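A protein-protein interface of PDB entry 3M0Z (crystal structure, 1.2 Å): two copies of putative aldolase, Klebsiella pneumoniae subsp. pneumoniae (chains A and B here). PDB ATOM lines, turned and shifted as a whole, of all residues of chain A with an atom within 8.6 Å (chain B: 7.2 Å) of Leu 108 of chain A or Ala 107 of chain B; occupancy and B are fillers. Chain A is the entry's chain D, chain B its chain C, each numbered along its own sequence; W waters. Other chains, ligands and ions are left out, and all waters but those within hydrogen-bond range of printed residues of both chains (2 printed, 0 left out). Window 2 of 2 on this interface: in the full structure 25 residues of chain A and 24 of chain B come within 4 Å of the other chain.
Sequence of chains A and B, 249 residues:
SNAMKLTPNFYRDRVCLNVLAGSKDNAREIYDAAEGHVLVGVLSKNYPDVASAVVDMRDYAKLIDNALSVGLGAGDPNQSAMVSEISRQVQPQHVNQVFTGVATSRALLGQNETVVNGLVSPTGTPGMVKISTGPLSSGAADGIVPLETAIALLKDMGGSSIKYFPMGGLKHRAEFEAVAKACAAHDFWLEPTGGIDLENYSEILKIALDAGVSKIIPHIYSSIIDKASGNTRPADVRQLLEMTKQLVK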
ATOM      1  N   VAL A  50      -0.221  -1.912   1.015  1.00  0.00           N
ATOM      2  CA  VAL A  50       0.114  -0.479   0.988  1.00  0.00           C
ATOM      3  C   VAL A  50       1.329  -0.244   0.094  1.00  0.00           C
ATOM      4  O   VAL A  50       1.332   0.679  -0.728  1.00  0.00           O
ATOM      5  CB  VAL A  50       0.338   0.076   2.424  1.00  0.00           C
ATOM      6  CG1 VAL A  50       0.986   1.479   2.413  1.00  0.00           C
ATOM      7  CG2 VAL A  50      -0.979   0.049   3.176  1.00  0.00           C
ATOM      8  N   SER A  80     -10.530   1.608   4.635  1.00  0.00           N
ATOM      9  CA  SER A  80     -10.205   2.889   5.242  1.00  0.00           C
ATOM     10  C   SER A  80      -8.778   2.955   5.771  1.00  0.00           C
ATOM     11  O   SER A  80      -8.072   3.948   5.490  1.00  0.00           O
ATOM     12  CB  SER A  80     -11.212   3.181   6.374  1.00  0.00           C
ATOM     13  OG  SER A  80     -10.937   4.424   7.008  1.00  0.00           O
ATOM     14  N   ALA A  81      -8.359   1.960   6.576  1.00  0.00           N
ATOM     15  CA  ALA A  81      -7.014   2.014   7.114  1.00  0.00           C
ATOM     16  C   ALA A  81      -5.948   2.018   6.029  1.00  0.00           C
ATOM     17  O   ALA A  81      -4.970   2.775   6.100  1.00  0.00           O
ATOM     18  CB  ALA A  81      -6.789   0.869   8.103  1.00  0.00           C
ATOM     19  N   MET A  82      -6.153   1.194   5.000  1.00  0.00           N
ATOM     20  CA  MET A  82      -5.184   1.139   3.917  1.00  0.00           C
ATOM     21  C   MET A  82      -5.087   2.478   3.205  1.00  0.00           C
ATOM     22  O   MET A  82      -3.996   2.933   2.869  1.00  0.00           O
ATOM     23  CB  MET A  82      -5.570   0.018   2.971  1.00  0.00           C
ATOM     24  CG  MET A  82      -4.564  -0.241   1.941  1.00  0.00           C
ATOM     25  SD  MET A  82      -5.082  -1.729   0.808  1.00  0.00           S
ATOM     26  CE  MET A  82      -3.761  -1.599  -0.544  1.00  0.00           C
ATOM     27  N   VAL A  83      -6.236   3.124   2.961  1.00  0.00           N
ATOM     28  CA  VAL A  83      -6.226   4.430   2.339  1.00  0.00           C
ATOM     29  C   VAL A  83      -5.413   5.448   3.173  1.00  0.00           C
ATOM     30  O   VAL A  83      -4.634   6.219   2.640  1.00  0.00           O
ATOM     31  CB  VAL A  83      -7.654   4.931   2.052  1.00  0.00           C
ATOM     32  CG1 VAL A  83      -7.688   6.435   1.761  1.00  0.00           C
ATOM     33  CG2 VAL A  83      -8.228   4.144   0.846  1.00  0.00           C
ATOM     34  N   SER A  84      -5.612   5.450   4.485  1.00  0.00           N
ATOM     35  CA  SER A  84      -4.854   6.371   5.340  1.00  0.00           C
ATOM     36  C   SER A  84      -3.337   6.124   5.216  1.00  0.00           C
ATOM     37  O   SER A  84      -2.567   7.075   5.114  1.00  0.00           O
ATOM     38  CB  SER A  84      -5.298   6.218   6.801  1.00  0.00           C
ATOM     39  OG  SER A  84      -6.630   6.640   6.940  1.00  0.00           O
ATOM     40  N   GLU A  85      -2.948   4.848   5.230  1.00  0.00           N
ATOM     41  CA  GLU A  85      -1.522   4.512   5.187  1.00  0.00           C
ATOM     42  C   GLU A  85      -0.932   4.829   3.806  1.00  0.00           C
ATOM     43  O   GLU A  85       0.184   5.353   3.698  1.00  0.00           O
ATOM     44  CB  GLU A  85      -1.329   3.047   5.523  1.00  0.00           C
ATOM     45  CG  GLU A  85      -1.607   2.813   6.982  1.00  0.00           C
ATOM     46  CD  GLU A  85      -1.992   1.382   7.309  1.00  0.00           C
ATOM     47  OE1 GLU A  85      -1.740   0.458   6.502  1.00  0.00           O
ATOM     48  OE2 GLU A  85      -2.534   1.169   8.400  1.00  0.00           O
ATOM     49  N   ILE A  86      -1.668   4.552   2.733  1.00  0.00           N
ATOM     50  CA  ILE A  86      -1.189   4.918   1.410  1.00  0.00           C
ATOM     51  C   ILE A  86      -0.974   6.433   1.306  1.00  0.00           C
ATOM     52  O   ILE A  86       0.057   6.904   0.792  1.00  0.00           O
ATOM     53  CB  ILE A  86      -2.192   4.461   0.327  1.00  0.00           C
ATOM     54  CG1 ILE A  86      -2.246   2.919   0.222  1.00  0.00           C
ATOM     55  CG2 ILE A  86      -1.878   5.103  -1.033  1.00  0.00           C
ATOM     56  CD1 ILE A  86      -3.457   2.431  -0.566  1.00  0.00           C
ATOM     57  N   SER A  87      -1.977   7.179   1.780  1.00  0.00           N
ATOM     58  CA  SER A  87      -1.939   8.612   1.614  1.00  0.00           C
ATOM     59  C   SER A  87      -0.776   9.242   2.347  1.00  0.00           C
ATOM     60  O   SER A  87      -0.256  10.276   1.900  1.00  0.00           O
ATOM     61  CB  SER A  87      -3.287   9.197   2.067  1.00  0.00           C
ATOM     62  OG  SER A  87      -4.362   8.660   1.255  1.00  0.00           O
ATOM     63  N   ARG A  88      -0.390   8.659   3.497  1.00  0.00           N
ATOM     64  CA  ARG A  88       0.754   9.163   4.241  1.00  0.00           C
ATOM     65  C   ARG A  88       1.988   9.292   3.332  1.00  0.00           C
ATOM     66  O   ARG A  88       2.681  10.296   3.367  1.00  0.00           O
ATOM     67  CB  ARG A  88       1.085   8.210   5.378  1.00  0.00           C
ATOM     68  CG  ARG A  88       2.381   8.612   6.099  1.00  0.00           C
ATOM     69  CD  ARG A  88       2.536   7.962   7.444  1.00  0.00           C
ATOM     70  NE  ARG A  88       2.429   6.510   7.333  1.00  0.00           N
ATOM     71  CZ  ARG A  88       2.290   5.674   8.355  1.00  0.00           C
ATOM     72  NH1 ARG A  88       2.264   6.116   9.619  1.00  0.00           N
ATOM     73  NH2 ARG A  88       2.178   4.384   8.114  1.00  0.00           N
ATOM     74  N   GLN A  89       2.233   8.275   2.511  1.00  0.00           N
ATOM     75  CA  GLN A  89       3.412   8.275   1.661  1.00  0.00           C
ATOM     76  C   GLN A  89       3.191   8.943   0.306  1.00  0.00           C
ATOM     77  O   GLN A  89       4.106   9.603  -0.236  1.00  0.00           O
ATOM     78  CB  GLN A  89       3.933   6.835   1.454  1.00  0.00           C
ATOM     79  CG  GLN A  89       4.607   6.269   2.728  1.00  0.00           C
ATOM     80  CD  GLN A  89       4.838   4.774   2.666  1.00  0.00           C
ATOM     81  OE1 GLN A  89       4.177   4.014   3.375  1.00  0.00           O
ATOM     82  NE2 GLN A  89       5.745   4.345   1.794  1.00  0.00           N
ATOM     83  N   VAL A  90       1.976   8.814  -0.245  1.00  0.00           N
ATOM     84  CA  VAL A  90       1.702   9.395  -1.571  1.00  0.00           C
ATOM     85  C   VAL A  90       1.584  10.924  -1.507  1.00  0.00           C
ATOM     86  O   VAL A  90       1.960  11.621  -2.451  1.00  0.00           O
ATOM     87  CB  VAL A  90       0.477   8.717  -2.232  1.00  0.00           C
ATOM     88  CG1 VAL A  90       0.028   9.430  -3.515  1.00  0.00           C
ATOM     89  CG2 VAL A  90       0.794   7.260  -2.527  1.00  0.00           C
ATOM     90  N   GLN A  91       1.038  11.454  -0.414  1.00  0.00           N
ATOM     91  CA  GLN A  91       0.801  12.899  -0.308  1.00  0.00           C
ATOM     92  C   GLN A  91       0.055  13.444  -1.527  1.00  0.00           C
ATOM     93  O   GLN A  91       0.527  14.371  -2.213  1.00  0.00           O
ATOM     94  CB  GLN A  91       2.139  13.628  -0.055  1.00  0.00           C
ATOM     95  CG  GLN A  91       2.799  13.228   1.273  1.00  0.00           C
ATOM     96  CD  GLN A  91       2.079  13.830   2.454  1.00  0.00           C
ATOM     97  OE1 GLN A  91       1.703  15.024   2.428  1.00  0.00           O
ATOM     98  NE2 GLN A  91       1.899  13.042   3.504  1.00  0.00           N
ATOM     99  N   GLN A  97     -12.529   9.189   2.341  1.00  0.00           N
ATOM    100  CA  GLN A  97     -12.612   8.471   3.603  1.00  0.00           C
ATOM    101  C   GLN A  97     -14.059   8.239   4.001  1.00  0.00           C
ATOM    102  O   GLN A  97     -14.994   8.962   3.623  1.00  0.00           O
ATOM    103  CB  GLN A  97     -11.880   9.184   4.755  1.00  0.00           C
ATOM    104  CG  GLN A  97     -10.437   8.718   4.881  1.00  0.00           C
ATOM    105  CD  GLN A  97     -10.314   7.222   5.134  1.00  0.00           C
ATOM    106  OE1 GLN A  97     -11.296   6.533   5.486  1.00  0.00           O
ATOM    107  NE2 GLN A  97      -9.093   6.716   4.990  1.00  0.00           N
ATOM    108  N   GLY A 101     -12.700   7.404   9.343  1.00  0.00           N
ATOM    109  CA  GLY A 101     -11.325   7.388   8.866  1.00  0.00           C
ATOM    110  C   GLY A 101     -10.752   8.772   8.578  1.00  0.00           C
ATOM    111  O   GLY A 101      -9.561   8.854   8.257  1.00  0.00           O
ATOM    112  N   VAL A 102     -11.583   9.818   8.621  1.00  0.00           N
ATOM    113  CA  VAL A 102     -11.137  11.167   8.279  1.00  0.00           C
ATOM    114  C   VAL A 102      -9.951  11.614   9.139  1.00  0.00           C
ATOM    115  O   VAL A 102      -8.909  12.056   8.613  1.00  0.00           O
ATOM    116  CB  VAL A 102     -12.307  12.149   8.379  1.00  0.00           C
ATOM    117  CG1 VAL A 102     -11.893  13.580   8.179  1.00  0.00           C
ATOM    118  CG2 VAL A 102     -13.412  11.751   7.370  1.00  0.00           C
ATOM    119  N   ALA A 103     -10.109  11.542  10.464  1.00  0.00           N
ATOM    120  CA  ALA A 103      -9.064  11.965  11.379  1.00  0.00           C
ATOM    121  C   ALA A 103      -7.793  11.125  11.232  1.00  0.00           C
ATOM    122  O   ALA A 103      -6.673  11.672  11.293  1.00  0.00           O
ATOM    123  CB  ALA A 103      -9.553  11.896  12.802  1.00  0.00           C
ATOM    124  N   THR A 104      -7.933   9.815  11.021  1.00  0.00           N
ATOM    125  CA  THR A 104      -6.739   8.991  10.818  1.00  0.00           C
ATOM    126  C   THR A 104      -5.970   9.447   9.585  1.00  0.00           C
ATOM    127  O   THR A 104      -4.750   9.578   9.612  1.00  0.00           O
ATOM    128  CB  THR A 104      -7.143   7.522  10.701  1.00  0.00           C
ATOM    129  OG1 THR A 104      -7.821   7.156  11.911  1.00  0.00           O
ATOM    130  CG2 THR A 104      -5.951   6.619  10.495  1.00  0.00           C
ATOM    131  N   SER A 105      -6.679   9.680   8.480  1.00  0.00           N
ATOM    132  CA  SER A 105      -6.012  10.156   7.275  1.00  0.00           C
ATOM    133  C   SER A 105      -5.363  11.519   7.480  1.00  0.00           C
ATOM    134  O   SER A 105      -4.220  11.730   7.080  1.00  0.00           O
ATOM    135  CB  SER A 105      -6.972  10.196   6.081  1.00  0.00           C
ATOM    136  OG  SER A 105      -7.198   8.879   5.585  1.00  0.00           O
ATOM    137  N   ARG A 106      -6.067  12.452   8.124  1.00  0.00           N
ATOM    138  CA  ARG A 106      -5.468  13.750   8.370  1.00  0.00           C
ATOM    139  C   ARG A 106      -4.200  13.594   9.198  1.00  0.00           C
ATOM    140  O   ARG A 106      -3.193  14.257   8.927  1.00  0.00           O
ATOM    141  CB  ARG A 106      -6.468  14.696   9.046  1.00  0.00           C
ATOM    142  CG  ARG A 106      -5.876  16.107   9.325  1.00  0.00           C
ATOM    143  CD  ARG A 106      -5.458  16.867   8.095  1.00  0.00           C
ATOM    144  NE  ARG A 106      -6.628  17.164   7.268  1.00  0.00           N
ATOM    145  CZ  ARG A 106      -6.633  17.391   5.956  1.00  0.00           C
ATOM    146  NH1 ARG A 106      -5.469  17.394   5.261  1.00  0.00           N
ATOM    147  NH2 ARG A 106      -7.782  17.673   5.345  1.00  0.00           N
ATOM    148  N   ALA A 107      -4.262  12.779  10.258  1.00  0.00           N
ATOM    149  CA  ALA A 107      -3.094  12.630  11.140  1.00  0.00           C
ATOM    150  C   ALA A 107      -1.912  12.034  10.373  1.00  0.00           C
ATOM    151  O   ALA A 107      -0.760  12.464  10.531  1.00  0.00           O
ATOM    152  CB  ALA A 107      -3.441  11.740  12.317  1.00  0.00           C
ATOM    153  N   LEU A 108      -2.164  11.035   9.538  1.00  0.00           N
ATOM    154  CA  LEU A 108      -1.087  10.394   8.796  1.00  0.00           C
ATOM    155  C   LEU A 108      -0.551  11.258   7.648  1.00  0.00           C
ATOM    156  O   LEU A 108       0.633  11.180   7.328  1.00  0.00           O
ATOM    157  CB  LEU A 108      -1.510   9.012   8.317  1.00  0.00           C
ATOM    158  CG  LEU A 108      -1.284   7.845   9.260  1.00  0.00           C
ATOM    159  CD1 LEU A 108      -1.644   8.051  10.665  1.00  0.00           C
ATOM    160  CD2 LEU A 108      -1.759   6.530   8.729  1.00  0.00           C
ATOM    161  N   LEU A 109      -1.393  12.103   7.061  1.00  0.00           N
ATOM    162  CA  LEU A 109      -0.915  13.059   6.067  1.00  0.00           C
ATOM    163  C   LEU A 109       0.066  14.049   6.661  1.00  0.00           C
ATOM    164  O   LEU A 109       1.047  14.401   5.989  1.00  0.00           O
ATOM    165  CB  LEU A 109      -2.094  13.823   5.443  1.00  0.00           C
ATOM    166  CG  LEU A 109      -2.897  13.025   4.429  1.00  0.00           C
ATOM    167  CD1 LEU A 109      -4.316  13.608   4.249  1.00  0.00           C
ATOM    168  CD2 LEU A 109      -2.151  12.992   3.085  1.00  0.00           C
ATOM    169  N   GLY A 110      -0.209  14.510   7.880  1.00  0.00           N
ATOM    170  CA  GLY A 110       0.685  15.446   8.556  1.00  0.00           C
ATOM    171  C   GLY A 110       0.545  16.898   8.139  1.00  0.00           C
ATOM    172  O   GLY A 110       1.303  17.732   8.616  1.00  0.00           O
ATOM    173  N   GLN A 111      -0.421  17.210   7.279  1.00  0.00           N
ATOM    174  CA  GLN A 111      -0.641  18.562   6.819  1.00  0.00           C
ATOM    175  C   GLN A 111      -2.112  18.732   6.516  1.00  0.00           C
ATOM    176  O   GLN A 111      -2.871  17.753   6.401  1.00  0.00           O
ATOM    177  CB  GLN A 111       0.283  18.929   5.622  1.00  0.00           C
ATOM    178  CG  GLN A 111       0.486  17.832   4.581  1.00  0.00           C
ATOM    179  CD  GLN A 111      -0.713  17.657   3.624  1.00  0.00           C
ATOM    180  OE1 GLN A 111      -1.628  18.497   3.555  1.00  0.00           O
ATOM    181  NE2 GLN A 111      -0.724  16.538   2.919  1.00  0.00           N
ATOM    182  N   VAL A 116      -9.516  15.979   2.373  1.00  0.00           N
ATOM    183  CA  VAL A 116      -9.970  14.678   2.886  1.00  0.00           C
ATOM    184  C   VAL A 116     -11.500  14.740   3.019  1.00  0.00           C
ATOM    185  O   VAL A 116     -12.031  15.535   3.815  1.00  0.00           O
ATOM    186  CB  VAL A 116      -9.356  14.342   4.250  1.00  0.00           C
ATOM    187  CG1 VAL A 116      -9.833  12.989   4.730  1.00  0.00           C
ATOM    188  CG2 VAL A 116      -7.799  14.337   4.138  1.00  0.00           C
ATOM    189  N   ARG B  88       1.223  11.144  22.137  1.00  0.00           N
ATOM    190  CA  ARG B  88       2.164  10.641  21.133  1.00  0.00           C
ATOM    191  C   ARG B  88       3.573  10.626  21.727  1.00  0.00           C
ATOM    192  O   ARG B  88       4.337   9.661  21.547  1.00  0.00           O
ATOM    193  CB  ARG B  88       2.123  11.581  19.946  1.00  0.00           C
ATOM    194  CG  ARG B  88       3.121  11.408  18.886  1.00  0.00           C
ATOM    195  CD  ARG B  88       3.022  12.698  18.027  1.00  0.00           C
ATOM    196  NE  ARG B  88       3.358  12.368  16.701  1.00  0.00           N
ATOM    197  CZ  ARG B  88       3.142  13.135  15.650  1.00  0.00           C
ATOM    198  NH1 ARG B  88       3.472  12.654  14.483  1.00  0.00           N
ATOM    199  NH2 ARG B  88       2.611  14.359  15.775  1.00  0.00           N
ATOM    200  N   GLY B 101     -11.573  13.185  18.901  1.00  0.00           N
ATOM    201  CA  GLY B 101     -10.121  13.089  19.105  1.00  0.00           C
ATOM    202  C   GLY B 101      -9.607  11.687  19.271  1.00  0.00           C
ATOM    203  O   GLY B 101      -8.391  11.503  19.337  1.00  0.00           O
ATOM    204  N   VAL B 102     -10.493  10.684  19.330  1.00  0.00           N
ATOM    205  CA  VAL B 102     -10.095   9.299  19.590  1.00  0.00           C
ATOM    206  C   VAL B 102      -9.160   8.796  18.480  1.00  0.00           C
ATOM    207  O   VAL B 102      -8.079   8.287  18.742  1.00  0.00           O
ATOM    208  CB  VAL B 102     -11.348   8.411  19.693  1.00  0.00           C
ATOM    209  CG1 VAL B 102     -10.949   6.947  19.759  1.00  0.00           C
ATOM    210  CG2 VAL B 102     -12.167   8.825  20.911  1.00  0.00           C
ATOM    211  N   ALA B 103      -9.581   8.975  17.228  1.00  0.00           N
ATOM    212  CA  ALA B 103      -8.796   8.470  16.096  1.00  0.00           C
ATOM    213  C   ALA B 103      -7.454   9.193  15.989  1.00  0.00           C
ATOM    214  O   ALA B 103      -6.418   8.581  15.684  1.00  0.00           O
ATOM    215  CB  ALA B 103      -9.538   8.556  14.795  1.00  0.00           C
ATOM    216  N   THR B 104      -7.459  10.502  16.206  1.00  0.00           N
ATOM    217  CA  THR B 104      -6.205  11.265  16.165  1.00  0.00           C
ATOM    218  C   THR B 104      -5.235  10.762  17.206  1.00  0.00           C
ATOM    219  O   THR B 104      -4.058  10.508  16.932  1.00  0.00           O
ATOM    220  CB  THR B 104      -6.466  12.739  16.373  1.00  0.00           C
ATOM    221  OG1 THR B 104      -7.322  13.217  15.313  1.00  0.00           O
ATOM    222  CG2 THR B 104      -5.167  13.581  16.406  1.00  0.00           C
ATOM    223  N   SER B 105      -5.723  10.564  18.430  1.00  0.00           N
ATOM    224  CA  SER B 105      -4.841  10.028  19.468  1.00  0.00           C
ATOM    225  C   SER B 105      -4.340   8.640  19.102  1.00  0.00           C
ATOM    226  O   SER B 105      -3.160   8.359  19.263  1.00  0.00           O
ATOM    227  CB  SER B 105      -5.548  10.014  20.828  1.00  0.00           C
ATOM    228  OG  SER B 105      -5.547  11.329  21.408  1.00  0.00           O
ATOM    229  N   ARG B 106      -5.217   7.748  18.633  1.00  0.00           N
ATOM    230  CA  ARG B 106      -4.765   6.415  18.263  1.00  0.00           C
ATOM    231  C   ARG B 106      -3.692   6.481  17.175  1.00  0.00           C
ATOM    232  O   ARG B 106      -2.671   5.782  17.259  1.00  0.00           O
ATOM    233  CB  ARG B 106      -5.951   5.539  17.840  1.00  0.00           C
ATOM    234  CG  ARG B 106      -5.515   4.138  17.341  1.00  0.00           C
ATOM    235  CD  ARG B 106      -4.841   3.284  18.432  1.00  0.00           C
ATOM    236  NE  ARG B 106      -5.814   3.031  19.507  1.00  0.00           N
ATOM    237  CZ  ARG B 106      -5.513   2.755  20.777  1.00  0.00           C
ATOM    238  NH1 ARG B 106      -4.242   2.671  21.184  1.00  0.00           N
ATOM    239  NH2 ARG B 106      -6.495   2.519  21.634  1.00  0.00           N
ATOM    240  N   ALA B 107      -3.932   7.292  16.157  1.00  0.00           N
ATOM    241  CA  ALA B 107      -3.001   7.371  15.037  1.00  0.00           C
ATOM    242  C   ALA B 107      -1.648   7.897  15.507  1.00  0.00           C
ATOM    243  O   ALA B 107      -0.598   7.396  15.113  1.00  0.00           O
ATOM    244  CB  ALA B 107      -3.578   8.290  13.959  1.00  0.00           C
ATOM    245  N   LEU B 108      -1.645   8.920  16.351  1.00  0.00           N
ATOM    246  CA  LEU B 108      -0.382   9.494  16.784  1.00  0.00           C
ATOM    247  C   LEU B 108       0.314   8.632  17.825  1.00  0.00           C
ATOM    248  O   LEU B 108       1.549   8.630  17.878  1.00  0.00           O
ATOM    249  CB  LEU B 108      -0.590  10.912  17.317  1.00  0.00           C
ATOM    250  CG  LEU B 108      -1.092  11.934  16.240  1.00  0.00           C
ATOM    251  CD1 LEU B 108      -1.109  13.350  16.858  1.00  0.00           C
ATOM    252  CD2 LEU B 108      -0.298  11.911  14.939  1.00  0.00           C
ATOM    253  N   LEU B 109      -0.430   7.851  18.619  1.00  0.00           N
ATOM    254  CA  LEU B 109       0.191   6.888  19.531  1.00  0.00           C
ATOM    255  C   LEU B 109       1.013   5.869  18.753  1.00  0.00           C
ATOM    256  O   LEU B 109       2.069   5.437  19.221  1.00  0.00           O
ATOM    257  CB  LEU B 109      -0.862   6.175  20.383  1.00  0.00           C
ATOM    258  CG  LEU B 109      -1.386   6.997  21.559  1.00  0.00           C
ATOM    259  CD1 LEU B 109      -2.710   6.418  21.970  1.00  0.00           C
ATOM    260  CD2 LEU B 109      -0.361   6.970  22.704  1.00  0.00           C
ATOM    261  N   GLY B 110       0.514   5.456  17.577  1.00  0.00           N
ATOM    262  CA  GLY B 110       1.233   4.510  16.740  1.00  0.00           C
ATOM    263  C   GLY B 110       1.198   3.090  17.216  1.00  0.00           C
ATOM    264  O   GLY B 110       1.944   2.279  16.721  1.00  0.00           O
ATOM    265  N   GLN B 111       0.335   2.766  18.175  1.00  0.00           N
ATOM    266  CA  GLN B 111       0.186   1.386  18.653  1.00  0.00           C
ATOM    267  C   GLN B 111      -1.216   1.274  19.233  1.00  0.00           C
ATOM    268  O   GLN B 111      -1.903   2.277  19.482  1.00  0.00           O
ATOM    269  CB  GLN B 111       1.302   0.958  19.640  1.00  0.00           C
ATOM    270  CG  GLN B 111       1.734   2.042  20.651  1.00  0.00           C
ATOM    271  CD  GLN B 111       0.766   2.280  21.792  1.00  0.00           C
ATOM    272  OE1 GLN B 111      -0.132   1.489  22.051  1.00  0.00           O
ATOM    273  NE2 GLN B 111       0.983   3.399  22.509  1.00  0.00           N
ATOM    274  N   MET B 157     -12.858   4.071  15.113  1.00  0.00           N
ATOM    275  CA  MET B 157     -11.915   5.181  15.279  1.00  0.00           C
ATOM    276  C   MET B 157     -10.767   4.863  16.240  1.00  0.00           C
ATOM    277  O   MET B 157     -10.081   5.780  16.674  1.00  0.00           O
ATOM    278  CB  MET B 157     -12.679   6.407  15.740  1.00  0.00           C
ATOM    279  CG  MET B 157     -13.644   6.886  14.668  1.00  0.00           C
ATOM    280  SD  MET B 157     -14.570   8.550  14.999  1.00  0.00           S
ATOM    281  CE  MET B 157     -15.137   8.185  16.822  1.00  0.00           C
ATOM    282  N   GLY B 158     -10.591   3.582  16.579  1.00  0.00           N
ATOM    283  CA  GLY B 158      -9.412   3.174  17.371  1.00  0.00           C
ATOM    284  C   GLY B 158      -9.617   3.296  18.864  1.00  0.00           C
ATOM    285  O   GLY B 158      -8.651   3.167  19.612  1.00  0.00           O
HETATM  286  O   HOH W   1      -6.592   6.249  14.140  1.00  0.00           O
HETATM  287  O   HOH W   2      -6.333  13.967  12.900  1.00  0.00           O
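Of the printed residues of chain B, Thr 104 of chain A touches Ala 103.
Leu 108 of chain A touches just one residue of chain B: Ala 107.
Arg 88 of chain B touches none of the printed residues of chain A.
Printed residues of chain A within 4 Å of Ala 103 of chain B: Ala 103 and Thr 104.
Printed residues of chain A within 4 Å of Thr 104 of chain B: Ala 103.
Ala 107 of chain B touches just these residues of chain A: Ala 107 (3.8 Å) and Leu 108 (3.8 Å).
Gly 158 of chain B touches none of the printed residues of chain A.
The backbone NH of Ala 103 of chain B lies close to the backbone carbonyl oxygen of Met 157 of chain B.
Printed residues of chain A that touch a printed residue of chain B: Ala 103, Thr 104, Ala 107 and Leu 108.
Hydrophobic or aromatic side chains of chain A that line the printed part of chain B: Ala 103, Ala 107 and Leu 108.
Printed residues of chain B that touch a printed residue of chain A: Ala 103, Thr 104 and Ala 107.
Among the printed residues, no Asp or Glu carboxylate lies within 4 Å of a Lys or Arg side-chain nitrogen of the other chain.
Ala 103 of chain A touches its own counterpart, Ala 103 of chain B.
Ala 103 of chain A touches Thr 104 of chain B, and with the chains exchanged Thr 104 of chain A touches Ala 103 of chain B.
Ala 107 of chain A touches its own counterpart, Ala 107 of chain B.
Leu 108 of chain A touches Ala 107 of chain B, but with the chains exchanged Ala 107 of chain A does not touch Leu 108 of chain B (4.1 Å).
12 positions are printed for both chains.
Of the 5 pairs that touch across the chains among the printed residues, 4 have their exchanged pair printed and touching as well.
Water W1 lies within hydrogen-bond range of the side-chain hydroxyl (OG1) of Thr 104 of chain A (2.7 Å), the backbone carbonyl oxygen (O) of Ala 103 of chain B (2.8 Å) and the backbone NH (N) of Ala 107 of chain B (3.5 Å).
Water W2 lies within hydrogen-bond range of the side-chain hydroxyl (OG1) of Thr 104 of chain B and the backbone carbonyl oxygen (O) of Ala 103 of chain A.
Among the printed residues, merely in contact across the chains: Ala 103 of chain A with Ala 103 of chain B, Ala 103 of chain A with Thr 104 of chain B, Thr 104 of chain A with Ala 103 of chain B, Ala 107 of chain A with Ala 107 of chain B and Leu 108 of chain A with Ala 107 of chain B.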
